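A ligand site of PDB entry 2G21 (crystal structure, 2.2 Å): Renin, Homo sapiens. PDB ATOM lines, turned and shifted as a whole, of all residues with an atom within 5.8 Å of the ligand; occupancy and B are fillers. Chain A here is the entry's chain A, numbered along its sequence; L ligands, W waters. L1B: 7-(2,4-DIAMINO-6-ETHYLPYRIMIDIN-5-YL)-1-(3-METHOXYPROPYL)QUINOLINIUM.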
ATOM      1  N   THR A  11      -9.589  14.295  10.061  1.00  0.00           N
ATOM      2  CA  THR A  11      -9.963  13.974  11.436  1.00  0.00           C
ATOM      3  C   THR A  11     -10.695  15.114  12.147  1.00  0.00           C
ATOM      4  O   THR A  11     -11.342  14.901  13.161  1.00  0.00           O
ATOM      5  CB  THR A  11      -8.738  13.574  12.309  1.00  0.00           C
ATOM      6  OG1 THR A  11      -7.779  14.635  12.321  1.00  0.00           O
ATOM      7  CG2 THR A  11      -8.095  12.280  11.765  1.00  0.00           C
ATOM      8  N   GLN A  12     -10.586  16.323  11.609  1.00  0.00           N
ATOM      9  CA  GLN A  12     -11.247  17.471  12.194  1.00  0.00           C
ATOM     10  C   GLN A  12     -11.924  18.312  11.099  1.00  0.00           C
ATOM     11  O   GLN A  12     -11.281  18.660  10.103  1.00  0.00           O
ATOM     12  CB  GLN A  12     -10.232  18.321  12.957  1.00  0.00           C
ATOM     13  CG  GLN A  12      -9.602  17.597  14.154  1.00  0.00           C
ATOM     14  CD  GLN A  12      -8.504  18.404  14.830  1.00  0.00           C
ATOM     15  OE1 GLN A  12      -8.555  19.627  14.890  1.00  0.00           O
ATOM     16  NE2 GLN A  12      -7.502  17.704  15.370  1.00  0.00           N
ATOM     17  N   TYR A  13     -13.209  18.596  11.261  1.00  0.00           N
ATOM     18  CA  TYR A  13     -13.956  19.399  10.286  1.00  0.00           C
ATOM     19  C   TYR A  13     -14.589  20.581  11.023  1.00  0.00           C
ATOM     20  O   TYR A  13     -15.322  20.389  12.005  1.00  0.00           O
ATOM     21  CB  TYR A  13     -15.063  18.580   9.597  1.00  0.00           C
ATOM     22  CG  TYR A  13     -14.569  17.481   8.670  1.00  0.00           C
ATOM     23  CD1 TYR A  13     -14.110  16.267   9.167  1.00  0.00           C
ATOM     24  CD2 TYR A  13     -14.543  17.665   7.283  1.00  0.00           C
ATOM     25  CE1 TYR A  13     -13.648  15.270   8.327  1.00  0.00           C
ATOM     26  CE2 TYR A  13     -14.082  16.667   6.429  1.00  0.00           C
ATOM     27  CZ  TYR A  13     -13.632  15.472   6.946  1.00  0.00           C
ATOM     28  OH  TYR A  13     -13.182  14.477   6.114  1.00  0.00           O
ATOM     29  N   VAL A  29     -16.404  23.169  15.462  1.00  0.00           N
ATOM     30  CA  VAL A  29     -16.878  21.906  14.917  1.00  0.00           C
ATOM     31  C   VAL A  29     -18.393  21.820  15.164  1.00  0.00           C
ATOM     32  O   VAL A  29     -18.867  22.020  16.285  1.00  0.00           O
ATOM     33  CB  VAL A  29     -16.199  20.708  15.606  1.00  0.00           C
ATOM     34  CG1 VAL A  29     -16.754  19.411  15.062  1.00  0.00           C
ATOM     35  CG2 VAL A  29     -14.708  20.765  15.406  1.00  0.00           C
ATOM     36  N   ASP A  31     -21.129  19.763  15.851  1.00  0.00           N
ATOM     37  CA  ASP A  31     -21.190  18.439  16.445  1.00  0.00           C
ATOM     38  C   ASP A  31     -22.583  17.937  16.843  1.00  0.00           C
ATOM     39  O   ASP A  31     -23.184  18.452  17.785  1.00  0.00           O
ATOM     40  CB  ASP A  31     -20.236  18.480  17.649  1.00  0.00           C
ATOM     41  CG  ASP A  31     -20.369  17.322  18.583  1.00  0.00           C
ATOM     42  OD1 ASP A  31     -20.043  17.514  19.771  1.00  0.00           O
ATOM     43  OD2 ASP A  31     -20.775  16.220  18.150  1.00  0.00           O
ATOM     44  N   THR A  32     -23.083  16.941  16.117  1.00  0.00           N
ATOM     45  CA  THR A  32     -24.383  16.377  16.408  1.00  0.00           C
ATOM     46  C   THR A  32     -24.316  15.507  17.655  1.00  0.00           C
ATOM     47  O   THR A  32     -25.345  15.067  18.155  1.00  0.00           O
ATOM     48  CB  THR A  32     -24.918  15.494  15.256  1.00  0.00           C
ATOM     49  OG1 THR A  32     -23.984  14.442  14.967  1.00  0.00           O
ATOM     50  CG2 THR A  32     -25.163  16.337  14.014  1.00  0.00           C
ATOM     51  N   GLY A  33     -23.102  15.280  18.140  1.00  0.00           N
ATOM     52  CA  GLY A  33     -22.906  14.471  19.326  1.00  0.00           C
ATOM     53  C   GLY A  33     -22.997  15.211  20.653  1.00  0.00           C
ATOM     54  O   GLY A  33     -22.895  14.602  21.709  1.00  0.00           O
ATOM     55  N   SER A  34     -23.177  16.529  20.615  1.00  0.00           N
ATOM     56  CA  SER A  34     -23.299  17.310  21.849  1.00  0.00           C
ATOM     57  C   SER A  34     -24.379  18.372  21.613  1.00  0.00           C
ATOM     58  O   SER A  34     -24.884  18.496  20.505  1.00  0.00           O
ATOM     59  CB  SER A  34     -21.963  17.950  22.247  1.00  0.00           C
ATOM     60  OG  SER A  34     -21.530  18.923  21.316  1.00  0.00           O
ATOM     61  N   TYR A  76     -16.593  15.260  26.802  1.00  0.00           N
ATOM     62  CA  TYR A  76     -16.611  14.544  25.536  1.00  0.00           C
ATOM     63  C   TYR A  76     -15.830  13.248  25.750  1.00  0.00           C
ATOM     64  O   TYR A  76     -15.141  13.079  26.759  1.00  0.00           O
ATOM     65  CB  TYR A  76     -15.978  15.413  24.424  1.00  0.00           C
ATOM     66  CG  TYR A  76     -16.654  16.774  24.255  1.00  0.00           C
ATOM     67  CD1 TYR A  76     -16.216  17.883  24.956  1.00  0.00           C
ATOM     68  CD2 TYR A  76     -17.754  16.918  23.415  1.00  0.00           C
ATOM     69  CE1 TYR A  76     -16.844  19.099  24.823  1.00  0.00           C
ATOM     70  CE2 TYR A  76     -18.390  18.140  23.283  1.00  0.00           C
ATOM     71  CZ  TYR A  76     -17.933  19.225  23.991  1.00  0.00           C
ATOM     72  OH  TYR A  76     -18.565  20.436  23.866  1.00  0.00           O
ATOM     73  N   SER A  77     -15.946  12.322  24.804  1.00  0.00           N
ATOM     74  CA  SER A  77     -15.266  11.044  24.938  1.00  0.00           C
ATOM     75  C   SER A  77     -13.730  11.156  24.952  1.00  0.00           C
ATOM     76  O   SER A  77     -13.053  10.314  25.528  1.00  0.00           O
ATOM     77  CB  SER A  77     -15.693  10.103  23.806  1.00  0.00           C
ATOM     78  OG  SER A  77     -15.302  10.617  22.536  1.00  0.00           O
ATOM     79  N   THR A  78     -13.193  12.193  24.337  1.00  0.00           N
ATOM     80  CA  THR A  78     -11.747  12.352  24.281  1.00  0.00           C
ATOM     81  C   THR A  78     -11.189  13.498  25.120  1.00  0.00           C
ATOM     82  O   THR A  78      -9.982  13.793  25.076  1.00  0.00           O
ATOM     83  CB  THR A  78     -11.279  12.521  22.834  1.00  0.00           C
ATOM     84  OG1 THR A  78     -11.946  13.640  22.257  1.00  0.00           O
ATOM     85  CG2 THR A  78     -11.619  11.278  22.010  1.00  0.00           C
ATOM     86  N   GLY A  79     -12.051  14.152  25.883  1.00  0.00           N
ATOM     87  CA  GLY A  79     -11.587  15.262  26.688  1.00  0.00           C
ATOM     88  C   GLY A  79     -12.685  16.055  27.361  1.00  0.00           C
ATOM     89  O   GLY A  79     -13.868  15.834  27.115  1.00  0.00           O
ATOM     90  N   PRO A 111      -6.493  16.885  25.053  1.00  0.00           N
ATOM     91  CA  PRO A 111      -6.083  16.951  23.653  1.00  0.00           C
ATOM     92  C   PRO A 111      -6.247  18.301  22.943  1.00  0.00           C
ATOM     93  O   PRO A 111      -6.052  18.375  21.732  1.00  0.00           O
ATOM     94  CB  PRO A 111      -6.986  15.923  23.017  1.00  0.00           C
ATOM     95  CG  PRO A 111      -8.321  16.338  23.677  1.00  0.00           C
ATOM     96  CD  PRO A 111      -7.938  16.600  25.147  1.00  0.00           C
ATOM     97  N   PHE A 112      -6.617  19.361  23.652  1.00  0.00           N
ATOM     98  CA  PHE A 112      -6.884  20.602  22.936  1.00  0.00           C
ATOM     99  C   PHE A 112      -5.755  21.350  22.244  1.00  0.00           C
ATOM    100  O   PHE A 112      -6.019  22.235  21.433  1.00  0.00           O
ATOM    101  CB  PHE A 112      -7.724  21.519  23.812  1.00  0.00           C
ATOM    102  CG  PHE A 112      -9.080  20.936  24.100  1.00  0.00           C
ATOM    103  CD1 PHE A 112      -9.342  20.327  25.313  1.00  0.00           C
ATOM    104  CD2 PHE A 112     -10.024  20.875  23.096  1.00  0.00           C
ATOM    105  CE1 PHE A 112     -10.537  19.654  25.513  1.00  0.00           C
ATOM    106  CE2 PHE A 112     -11.216  20.207  23.288  1.00  0.00           C
ATOM    107  CZ  PHE A 112     -11.470  19.592  24.501  1.00  0.00           C
ATOM    108  N   LEU A 114      -4.009  19.830  20.350  1.00  0.00           N
ATOM    109  CA  LEU A 114      -4.085  19.108  19.088  1.00  0.00           C
ATOM    110  C   LEU A 114      -5.285  19.491  18.242  1.00  0.00           C
ATOM    111  O   LEU A 114      -5.435  18.978  17.139  1.00  0.00           O
ATOM    112  CB  LEU A 114      -4.121  17.610  19.352  1.00  0.00           C
ATOM    113  CG  LEU A 114      -2.889  17.045  20.059  1.00  0.00           C
ATOM    114  CD1 LEU A 114      -3.130  15.598  20.403  1.00  0.00           C
ATOM    115  CD2 LEU A 114      -1.666  17.200  19.158  1.00  0.00           C
ATOM    116  N   ALA A 115      -6.126  20.390  18.744  1.00  0.00           N
ATOM    117  CA  ALA A 115      -7.302  20.850  18.012  1.00  0.00           C
ATOM    118  C   ALA A 115      -6.996  22.045  17.115  1.00  0.00           C
ATOM    119  O   ALA A 115      -6.444  23.056  17.567  1.00  0.00           O
ATOM    120  CB  ALA A 115      -8.417  21.232  18.973  1.00  0.00           C
ATOM    121  N   PHE A 117      -9.454  23.556  15.607  1.00  0.00           N
ATOM    122  CA  PHE A 117     -10.601  24.430  15.865  1.00  0.00           C
ATOM    123  C   PHE A 117     -10.476  25.071  17.244  1.00  0.00           C
ATOM    124  O   PHE A 117      -9.686  24.600  18.064  1.00  0.00           O
ATOM    125  CB  PHE A 117     -11.918  23.642  15.811  1.00  0.00           C
ATOM    126  CG  PHE A 117     -11.944  22.440  16.735  1.00  0.00           C
ATOM    127  CD1 PHE A 117     -11.427  21.213  16.335  1.00  0.00           C
ATOM    128  CD2 PHE A 117     -12.511  22.543  18.004  1.00  0.00           C
ATOM    129  CE1 PHE A 117     -11.466  20.105  17.180  1.00  0.00           C
ATOM    130  CE2 PHE A 117     -12.545  21.441  18.856  1.00  0.00           C
ATOM    131  CZ  PHE A 117     -12.029  20.213  18.442  1.00  0.00           C
ATOM    132  N   GLY A 119     -13.533  26.122  19.159  1.00  0.00           N
ATOM    133  CA  GLY A 119     -14.661  25.690  19.948  1.00  0.00           C
ATOM    134  C   GLY A 119     -15.578  24.677  19.277  1.00  0.00           C
ATOM    135  O   GLY A 119     -15.222  24.070  18.264  1.00  0.00           O
ATOM    136  N   VAL A 120     -16.761  24.522  19.849  1.00  0.00           N
ATOM    137  CA  VAL A 120     -17.741  23.574  19.354  1.00  0.00           C
ATOM    138  C   VAL A 120     -19.138  24.162  19.351  1.00  0.00           C
ATOM    139  O   VAL A 120     -19.505  24.944  20.223  1.00  0.00           O
ATOM    140  CB  VAL A 120     -17.772  22.320  20.267  1.00  0.00           C
ATOM    141  CG1 VAL A 120     -18.794  21.321  19.743  1.00  0.00           C
ATOM    142  CG2 VAL A 120     -16.369  21.692  20.352  1.00  0.00           C
ATOM    143  N   TYR A 155     -18.879  15.938   4.327  1.00  0.00           N
ATOM    144  CA  TYR A 155     -17.467  15.933   4.733  1.00  0.00           C
ATOM    145  C   TYR A 155     -16.694  15.374   3.542  1.00  0.00           C
ATOM    146  O   TYR A 155     -16.880  14.224   3.157  1.00  0.00           O
ATOM    147  CB  TYR A 155     -17.215  15.035   5.943  1.00  0.00           C
ATOM    148  CG  TYR A 155     -17.537  15.639   7.309  1.00  0.00           C
ATOM    149  CD1 TYR A 155     -17.462  14.872   8.471  1.00  0.00           C
ATOM    150  CD2 TYR A 155     -17.920  16.978   7.423  1.00  0.00           C
ATOM    151  CE1 TYR A 155     -17.753  15.417   9.712  1.00  0.00           C
ATOM    152  CE2 TYR A 155     -18.213  17.522   8.650  1.00  0.00           C
ATOM    153  CZ  TYR A 155     -18.131  16.748   9.797  1.00  0.00           C
ATOM    154  OH  TYR A 155     -18.426  17.320  11.015  1.00  0.00           O
ATOM    155  N   ASP A 219     -22.544  10.775  14.766  1.00  0.00           N
ATOM    156  CA  ASP A 219     -21.817  11.888  15.349  1.00  0.00           C
ATOM    157  C   ASP A 219     -20.872  12.678  14.431  1.00  0.00           C
ATOM    158  O   ASP A 219     -19.774  12.215  14.109  1.00  0.00           O
ATOM    159  CB  ASP A 219     -21.026  11.326  16.552  1.00  0.00           C
ATOM    160  CG  ASP A 219     -20.516  12.413  17.484  1.00  0.00           C
ATOM    161  OD1 ASP A 219     -19.895  12.053  18.504  1.00  0.00           O
ATOM    162  OD2 ASP A 219     -20.735  13.604  17.215  1.00  0.00           O
ATOM    163  N   THR A 220     -21.293  13.876  14.046  1.00  0.00           N
ATOM    164  CA  THR A 220     -20.481  14.726  13.173  1.00  0.00           C
ATOM    165  C   THR A 220     -19.252  15.302  13.902  1.00  0.00           C
ATOM    166  O   THR A 220     -18.322  15.809  13.275  1.00  0.00           O
ATOM    167  CB  THR A 220     -21.289  15.911  12.628  1.00  0.00           C
ATOM    168  OG1 THR A 220     -21.749  16.708  13.732  1.00  0.00           O
ATOM    169  CG2 THR A 220     -22.489  15.419  11.799  1.00  0.00           C
ATOM    170  N   GLY A 221     -19.264  15.229  15.236  1.00  0.00           N
ATOM    171  CA  GLY A 221     -18.152  15.726  16.035  1.00  0.00           C
ATOM    172  C   GLY A 221     -17.133  14.653  16.360  1.00  0.00           C
ATOM    173  O   GLY A 221     -16.166  14.912  17.100  1.00  0.00           O
ATOM    174  N   ALA A 222     -17.327  13.446  15.830  1.00  0.00           N
ATOM    175  CA  ALA A 222     -16.406  12.350  16.064  1.00  0.00           C
ATOM    176  C   ALA A 222     -15.573  12.081  14.791  1.00  0.00           C
ATOM    177  O   ALA A 222     -16.110  12.056  13.688  1.00  0.00           O
ATOM    178  CB  ALA A 222     -17.178  11.091  16.453  1.00  0.00           C
ATOM    179  N   SER A 223     -14.267  11.885  14.955  1.00  0.00           N
ATOM    180  CA  SER A 223     -13.387  11.641  13.827  1.00  0.00           C
ATOM    181  C   SER A 223     -13.568  10.294  13.151  1.00  0.00           C
ATOM    182  O   SER A 223     -13.458  10.188  11.923  1.00  0.00           O
ATOM    183  CB  SER A 223     -11.922  11.749  14.228  1.00  0.00           C
ATOM    184  OG  SER A 223     -11.583  13.051  14.636  1.00  0.00           O
ATOM    185  N   ALA A 310     -16.877  10.951  11.196  1.00  0.00           N
ATOM    186  CA  ALA A 310     -16.370  11.432   9.915  1.00  0.00           C
ATOM    187  C   ALA A 310     -16.028  10.322   8.927  1.00  0.00           C
ATOM    188  O   ALA A 310     -16.210  10.491   7.732  1.00  0.00           O
ATOM    189  CB  ALA A 310     -15.163  12.323  10.145  1.00  0.00           C
HETATM  190  C1  L1B L   1     -15.789  14.375  20.705  1.00  0.00           C
HETATM  191  N1  L1B L   1     -17.049  13.907  20.481  1.00  0.00           N
HETATM  192  C2  L1B L   1     -17.985  14.828  20.155  1.00  0.00           C
HETATM  193  N2  L1B L   1     -17.748  16.131  20.043  1.00  0.00           N
HETATM  194  C3  L1B L   1     -16.492  16.612  20.259  1.00  0.00           C
HETATM  195  C4  L1B L   1     -15.420  15.744  20.587  1.00  0.00           C
HETATM  196  N3  L1B L   1     -14.873  13.445  21.054  1.00  0.00           N
HETATM  197  N4  L1B L   1     -19.244  14.422  19.920  1.00  0.00           N
HETATM  198  C5  L1B L   1     -16.341  18.109  20.094  1.00  0.00           C
HETATM  199  C6  L1B L   1     -16.282  18.503  18.612  1.00  0.00           C
HETATM  200  C7  L1B L   1     -13.312  16.753  21.692  1.00  0.00           C
HETATM  201  C8  L1B L   1     -11.943  17.134  21.567  1.00  0.00           C
HETATM  202  C9  L1B L   1     -11.224  16.930  20.353  1.00  0.00           C
HETATM  203  C10 L1B L   1     -11.902  16.345  19.223  1.00  0.00           C
HETATM  204  C11 L1B L   1     -13.270  15.981  19.410  1.00  0.00           C
HETATM  205  C12 L1B L   1     -13.987  16.170  20.590  1.00  0.00           C
HETATM  206  C13 L1B L   1      -9.774  17.363  20.305  1.00  0.00           C
HETATM  207  C14 L1B L   1      -9.030  17.143  18.977  1.00  0.00           C
HETATM  208  C15 L1B L   1      -9.801  16.492  17.808  1.00  0.00           C
HETATM  209  N5  L1B L   1     -11.227  16.121  17.999  1.00  0.00           N
HETATM  210  C16 L1B L   1     -11.878  15.489  16.814  1.00  0.00           C
HETATM  211  C17 L1B L   1     -12.668  16.587  16.068  1.00  0.00           C
HETATM  212  C18 L1B L   1     -13.785  16.130  15.111  1.00  0.00           C
HETATM  213  O1  L1B L   1     -14.068  16.913  13.953  1.00  0.00           O
HETATM  214  C19 L1B L   1     -15.132  16.317  13.195  1.00  0.00           C
HETATM  215  O   HOH W   1     -18.071  12.651  22.697  1.00  0.00           O
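The side-chain carboxylate (OD1) of Asp 31 sits at hydrogen-bond distance from a nitrogen (N2) of the ligand, at 2.7 Å. OD1 of Asp 219 is in hydrogen-bond range of N4 of the ligand. A nitrogen (N3) of the ligand is in hydrogen-bond range of the side-chain hydroxyl of Thr 78. The side-chain hydroxyl (OG) of Ser 77 sits at hydrogen-bond distance from a nitrogen (N3) of the ligand (3.2 Å). The backbone NH (N) of Tyr 13 is in hydrogen-bond range of an oxygen (O1) of the ligand, at 3.3 Å.
The side-chain carboxylate (OD2) of Asp 31 lies close to the backbone NH (N) of Gly 221 (3.4 Å). The side-chain carboxylate (OD2) of Asp 31 lies within hydrogen-bond range of the backbone NH (N) of Gly 33, 2.5 Å away. The backbone NH of Gly 221 sits at hydrogen-bond distance from the side-chain carboxylate of Asp 219 (3.0 Å). OD2 of Asp 219 lies within hydrogen-bond range of N of Gly 33 (3.0 Å). The backbone carbonyl oxygen of Thr 220 sits at hydrogen-bond distance from the side-chain hydroxyl of Tyr 155, at 2.7 Å. The side-chain hydroxyl of Thr 220 sits at hydrogen-bond distance from the backbone NH of Thr 32, at 2.7 Å. NE2 of Gln 12 is in hydrogen-bond range of O of Leu 114 (3.0 Å). The backbone NH (N) of Val 29 is in hydrogen-bond range of the backbone carbonyl oxygen (O) of Gly 119.
The backbone carbonyl oxygen (O) of Thr 11 sits close to an oxygen (O1) of the ligand (3.5 Å). Residues that only touch the ligand: Thr 220 (3.2 Å), Ser 223 (3.3 Å), Gly 221 (3.3 Å), Gln 12 (3.4 Å), Tyr 76 (3.4 Å), Val 120 (3.6 Å), Phe 112 (3.6 Å), Val 29 (3.7 Å), Gly 33 (3.7 Å), Pro 111 (3.8 Å) and Phe 117 (3.9 Å).
Water W1 lies within hydrogen-bond range of a nitrogen (N1) of the ligand (2.7 Å) and the backbone NH (N) of Ser 77 (3.0 Å).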
